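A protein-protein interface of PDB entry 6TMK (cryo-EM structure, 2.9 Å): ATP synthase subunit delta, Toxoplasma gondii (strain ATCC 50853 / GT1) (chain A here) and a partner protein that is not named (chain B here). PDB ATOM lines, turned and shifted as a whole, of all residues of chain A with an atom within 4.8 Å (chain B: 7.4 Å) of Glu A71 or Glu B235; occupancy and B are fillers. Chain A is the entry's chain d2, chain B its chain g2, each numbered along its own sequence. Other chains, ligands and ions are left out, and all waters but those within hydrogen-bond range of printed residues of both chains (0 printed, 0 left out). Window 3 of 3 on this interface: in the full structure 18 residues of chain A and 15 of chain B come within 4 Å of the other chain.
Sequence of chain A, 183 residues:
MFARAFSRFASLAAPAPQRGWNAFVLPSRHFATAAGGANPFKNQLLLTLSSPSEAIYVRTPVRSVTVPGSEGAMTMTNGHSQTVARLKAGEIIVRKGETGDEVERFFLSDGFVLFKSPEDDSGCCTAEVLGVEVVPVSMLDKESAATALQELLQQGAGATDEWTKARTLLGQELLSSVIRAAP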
ATOM      1  N   GLY A  69      14.224  34.273  -3.712  1.00  0.00           N
ATOM      2  CA  GLY A  69      14.093  32.868  -3.383  1.00  0.00           C
ATOM      3  C   GLY A  69      14.180  31.988  -4.615  1.00  0.00           C
ATOM      4  O   GLY A  69      14.116  32.435  -5.759  1.00  0.00           O
ATOM      5  N   SER A  70      14.330  30.687  -4.360  1.00  0.00           N
ATOM      6  CA  SER A  70      14.495  29.741  -5.458  1.00  0.00           C
ATOM      7  C   SER A  70      13.213  29.613  -6.269  1.00  0.00           C
ATOM      8  O   SER A  70      13.259  29.445  -7.492  1.00  0.00           O
ATOM      9  CB  SER A  70      14.921  28.380  -4.912  1.00  0.00           C
ATOM     10  OG  SER A  70      14.740  27.363  -5.880  1.00  0.00           O
ATOM     11  N   GLU A  71      12.060  29.691  -5.606  1.00  0.00           N
ATOM     12  CA  GLU A  71      10.791  29.718  -6.324  1.00  0.00           C
ATOM     13  C   GLU A  71      10.591  31.066  -7.003  1.00  0.00           C
ATOM     14  O   GLU A  71      10.427  31.146  -8.227  1.00  0.00           O
ATOM     15  CB  GLU A  71       9.641  29.418  -5.361  1.00  0.00           C
ATOM     16  CG  GLU A  71       9.774  28.083  -4.650  1.00  0.00           C
ATOM     17  CD  GLU A  71       9.739  26.906  -5.604  1.00  0.00           C
ATOM     18  OE1 GLU A  71       9.202  27.061  -6.721  1.00  0.00           O
ATOM     19  OE2 GLU A  71      10.252  25.827  -5.240  1.00  0.00           O
ATOM     20  N   GLY A  72      10.603  32.139  -6.219  1.00  0.00           N
ATOM     21  CA  GLY A  72      10.510  33.485  -6.751  1.00  0.00           C
ATOM     22  C   GLY A  72      10.920  34.477  -5.689  1.00  0.00           C
ATOM     23  O   GLY A  72      11.117  34.127  -4.523  1.00  0.00           O
ATOM     24  N   ALA A  73      11.044  35.732  -6.108  1.00  0.00           N
ATOM     25  CA  ALA A  73      11.383  36.785  -5.165  1.00  0.00           C
ATOM     26  C   ALA A  73      10.289  36.930  -4.115  1.00  0.00           C
ATOM     27  O   ALA A  73       9.120  36.618  -4.354  1.00  0.00           O
ATOM     28  CB  ALA A  73      11.594  38.109  -5.896  1.00  0.00           C
ATOM     29  N   MET A  74      10.683  37.407  -2.939  1.00  0.00           N
ATOM     30  CA  MET A  74       9.742  37.630  -1.853  1.00  0.00           C
ATOM     31  C   MET A  74      10.365  38.587  -0.852  1.00  0.00           C
ATOM     32  O   MET A  74      11.585  38.766  -0.810  1.00  0.00           O
ATOM     33  CB  MET A  74       9.342  36.321  -1.175  1.00  0.00           C
ATOM     34  CG  MET A  74      10.470  35.595  -0.477  1.00  0.00           C
ATOM     35  SD  MET A  74       9.926  34.007   0.173  1.00  0.00           S
ATOM     36  CE  MET A  74      11.447  33.398   0.881  1.00  0.00           C
ATOM     37  N   THR A  83      10.571  30.835   8.664  1.00  0.00           N
ATOM     38  CA  THR A  83      10.713  30.160   7.385  1.00  0.00           C
ATOM     39  C   THR A  83      12.182  30.029   7.027  1.00  0.00           C
ATOM     40  O   THR A  83      13.036  30.782   7.502  1.00  0.00           O
ATOM     41  CB  THR A  83       9.972  30.909   6.269  1.00  0.00           C
ATOM     42  OG1 THR A  83      10.016  30.140   5.061  1.00  0.00           O
ATOM     43  CG2 THR A  83      10.606  32.269   6.019  1.00  0.00           C
ATOM     44  N   VAL A  84      12.456  29.049   6.172  1.00  0.00           N
ATOM     45  CA  VAL A  84      13.760  28.848   5.558  1.00  0.00           C
ATOM     46  C   VAL A  84      13.552  28.761   4.056  1.00  0.00           C
ATOM     47  O   VAL A  84      12.554  28.200   3.592  1.00  0.00           O
ATOM     48  CB  VAL A  84      14.450  27.575   6.086  1.00  0.00           C
ATOM     49  CG1 VAL A  84      15.807  27.399   5.436  1.00  0.00           C
ATOM     50  CG2 VAL A  84      14.571  27.631   7.593  1.00  0.00           C
ATOM     51  N   ALA A  85      14.487  29.319   3.294  1.00  0.00           N
ATOM     52  CA  ALA A  85      14.363  29.310   1.848  1.00  0.00           C
ATOM     53  C   ALA A  85      15.745  29.296   1.219  1.00  0.00           C
ATOM     54  O   ALA A  85      16.708  29.830   1.774  1.00  0.00           O
ATOM     55  CB  ALA A  85      13.565  30.516   1.344  1.00  0.00           C
ATOM     56  N   LYS A  88      18.651  31.589  -5.423  1.00  0.00           N
ATOM     57  CA  LYS A  88      19.178  31.183  -6.717  1.00  0.00           C
ATOM     58  C   LYS A  88      20.103  32.229  -7.319  1.00  0.00           C
ATOM     59  O   LYS A  88      21.209  31.901  -7.759  1.00  0.00           O
ATOM     60  CB  LYS A  88      18.030  30.881  -7.696  1.00  0.00           C
ATOM     61  CG  LYS A  88      17.095  32.048  -7.976  1.00  0.00           C
ATOM     62  CD  LYS A  88      15.868  31.599  -8.756  1.00  0.00           C
ATOM     63  CE  LYS A  88      14.939  32.762  -9.063  1.00  0.00           C
ATOM     64  NZ  LYS A  88      13.691  32.320  -9.747  1.00  0.00           N
ATOM     65  N   PHE B 232       9.262  25.579  11.321  1.00  0.00           N
ATOM     66  CA  PHE B 232       9.859  26.351  10.243  1.00  0.00           C
ATOM     67  C   PHE B 232       9.189  26.021   8.916  1.00  0.00           C
ATOM     68  O   PHE B 232       8.862  24.863   8.641  1.00  0.00           O
ATOM     69  CB  PHE B 232      11.358  26.067  10.140  1.00  0.00           C
ATOM     70  CG  PHE B 232      12.196  26.891  11.070  1.00  0.00           C
ATOM     71  CD1 PHE B 232      12.403  26.487  12.376  1.00  0.00           C
ATOM     72  CD2 PHE B 232      12.772  28.072  10.639  1.00  0.00           C
ATOM     73  CE1 PHE B 232      13.174  27.243  13.232  1.00  0.00           C
ATOM     74  CE2 PHE B 232      13.542  28.832  11.491  1.00  0.00           C
ATOM     75  CZ  PHE B 232      13.744  28.417  12.790  1.00  0.00           C
ATOM     76  N   GLU B 233       8.989  27.051   8.100  1.00  0.00           N
ATOM     77  CA  GLU B 233       8.490  26.893   6.739  1.00  0.00           C
ATOM     78  C   GLU B 233       9.673  26.797   5.784  1.00  0.00           C
ATOM     79  O   GLU B 233      10.491  27.719   5.710  1.00  0.00           O
ATOM     80  CB  GLU B 233       7.594  28.067   6.355  1.00  0.00           C
ATOM     81  CG  GLU B 233       6.286  28.133   7.114  1.00  0.00           C
ATOM     82  CD  GLU B 233       5.449  29.330   6.711  1.00  0.00           C
ATOM     83  OE1 GLU B 233       5.657  29.852   5.595  1.00  0.00           O
ATOM     84  OE2 GLU B 233       4.592  29.758   7.511  1.00  0.00           O
ATOM     85  N   PHE B 234       9.758  25.696   5.049  1.00  0.00           N
ATOM     86  CA  PHE B 234      10.800  25.503   4.050  1.00  0.00           C
ATOM     87  C   PHE B 234      10.234  25.822   2.674  1.00  0.00           C
ATOM     88  O   PHE B 234       9.244  25.219   2.249  1.00  0.00           O
ATOM     89  CB  PHE B 234      11.341  24.075   4.101  1.00  0.00           C
ATOM     90  CG  PHE B 234      12.124  23.774   5.345  1.00  0.00           C
ATOM     91  CD1 PHE B 234      11.485  23.630   6.564  1.00  0.00           C
ATOM     92  CD2 PHE B 234      13.502  23.651   5.301  1.00  0.00           C
ATOM     93  CE1 PHE B 234      12.204  23.358   7.710  1.00  0.00           C
ATOM     94  CE2 PHE B 234      14.222  23.380   6.445  1.00  0.00           C
ATOM     95  CZ  PHE B 234      13.573  23.234   7.649  1.00  0.00           C
ATOM     96  N   GLU B 235      10.864  26.777   1.981  1.00  0.00           N
ATOM     97  CA  GLU B 235      10.258  27.312   0.762  1.00  0.00           C
ATOM     98  C   GLU B 235      10.208  26.258  -0.334  1.00  0.00           C
ATOM     99  O   GLU B 235       9.120  26.027  -0.892  1.00  0.00           O
ATOM    100  CB  GLU B 235      11.008  28.573   0.322  1.00  0.00           C
ATOM    101  CG  GLU B 235      10.622  29.095  -1.053  1.00  0.00           C
ATOM    102  CD  GLU B 235       9.152  29.447  -1.149  1.00  0.00           C
ATOM    103  OE1 GLU B 235       8.519  29.654  -0.092  1.00  0.00           O
ATOM    104  OE2 GLU B 235       8.630  29.526  -2.281  1.00  0.00           O
ATOM    105  N   PRO B 236      11.302  25.591  -0.694  1.00  0.00           N
ATOM    106  CA  PRO B 236      11.181  24.240  -1.244  1.00  0.00           C
ATOM    107  C   PRO B 236      10.836  23.251  -0.144  1.00  0.00           C
ATOM    108  O   PRO B 236      11.103  23.471   1.039  1.00  0.00           O
ATOM    109  CB  PRO B 236      12.566  23.954  -1.835  1.00  0.00           C
ATOM    110  CG  PRO B 236      13.275  25.254  -1.859  1.00  0.00           C
ATOM    111  CD  PRO B 236      12.677  26.099  -0.792  1.00  0.00           C
ATOM    112  N   GLU B 237      10.222  22.144  -0.551  1.00  0.00           N
ATOM    113  CA  GLU B 237       9.768  21.171   0.426  1.00  0.00           C
ATOM    114  C   GLU B 237      10.972  20.614   1.190  1.00  0.00           C
ATOM    115  O   GLU B 237      12.114  20.629   0.712  1.00  0.00           O
ATOM    116  CB  GLU B 237       8.965  20.078  -0.293  1.00  0.00           C
ATOM    117  CG  GLU B 237       8.124  19.143   0.576  1.00  0.00           C
ATOM    118  CD  GLU B 237       8.938  18.173   1.392  1.00  0.00           C
ATOM    119  OE1 GLU B 237      10.044  17.810   0.945  1.00  0.00           O
ATOM    120  OE2 GLU B 237       8.475  17.768   2.480  1.00  0.00           O
ATOM    121  N   LYS B 238      10.699  20.129   2.403  1.00  0.00           N
ATOM    122  CA  LYS B 238      11.777  19.740   3.306  1.00  0.00           C
ATOM    123  C   LYS B 238      12.649  18.643   2.708  1.00  0.00           C
ATOM    124  O   LYS B 238      13.878  18.698   2.807  1.00  0.00           O
ATOM    125  CB  LYS B 238      11.198  19.290   4.645  1.00  0.00           C
ATOM    126  CG  LYS B 238      12.238  19.135   5.731  1.00  0.00           C
ATOM    127  CD  LYS B 238      11.631  18.654   7.029  1.00  0.00           C
ATOM    128  CE  LYS B 238      10.908  19.773   7.748  1.00  0.00           C
ATOM    129  NZ  LYS B 238      10.391  19.337   9.072  1.00  0.00           N
ATOM    130  N   VAL B 241      14.974  20.244   0.060  1.00  0.00           N
ATOM    131  CA  VAL B 241      15.938  21.239   0.522  1.00  0.00           C
ATOM    132  C   VAL B 241      16.867  20.710   1.610  1.00  0.00           C
ATOM    133  O   VAL B 241      17.880  21.362   1.915  1.00  0.00           O
ATOM    134  CB  VAL B 241      15.213  22.503   1.030  1.00  0.00           C
ATOM    135  CG1 VAL B 241      14.566  22.235   2.372  1.00  0.00           C
ATOM    136  CG2 VAL B 241      16.171  23.678   1.114  1.00  0.00           C
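Of the 8 printed residues of chain B, 4 touch a printed residue of chain A.
Printed residues of chain B that touch a printed residue of chain A: Phe B232, Glu B233, Phe B234 and Glu B235.
Hydrophobic or aromatic side chains of chain B within 4 Å of the printed part of chain A: Phe B232.
Among the printed residues, no Asp or Glu carboxylate lies within 4 Å of a Lys or Arg side-chain nitrogen of the other chain.
Of chain B, only Glu B235 comes within 4 Å of Glu A71.
Printed residues of chain B within 4 Å of Val A84: Phe B232 (3.6 Å), Glu B233 (2.4 Å), Phe B234 (3.2 Å) and Glu B235 (2.7 Å).
Printed residues of chain B within 4 Å of Ala A85: Glu B235 (3.4 Å).
Printed residues of chain A within 4 Å of Glu B233: Thr A83 and Val A84.
Of the printed residues of chain A, Phe B234 touches Val A84 (3.2 Å).
Glu B235 touches just these residues of chain A: Glu A71 (3.0 Å), Val A84 (2.7 Å) and Ala A85 (3.4 Å).
The nearest residue of chain B that does not touch Glu A71 is Pro B236 (4.4 Å).
OG1 of Thr A83 sits at hydrogen-bond distance from O of Glu B233, at 2.6 Å.
The backbone carbonyl oxygen of Glu B233 sits at hydrogen-bond distance from the backbone NH of Val A84, at 2.4 Å.
The backbone carbonyl oxygen of Val A84 sits at hydrogen-bond distance from the backbone NH of Glu B235.
Glu A71 touches Glu B235 (CG to OE2, 3.0 Å).
Val A84 touches Phe B232 (CG2 to CD2, 3.6 Å).
Val A84 touches Phe B234 (O to CA, 3.2 Å).
Ala A85 touches Glu B235 (CB to CB, 3.4 Å).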
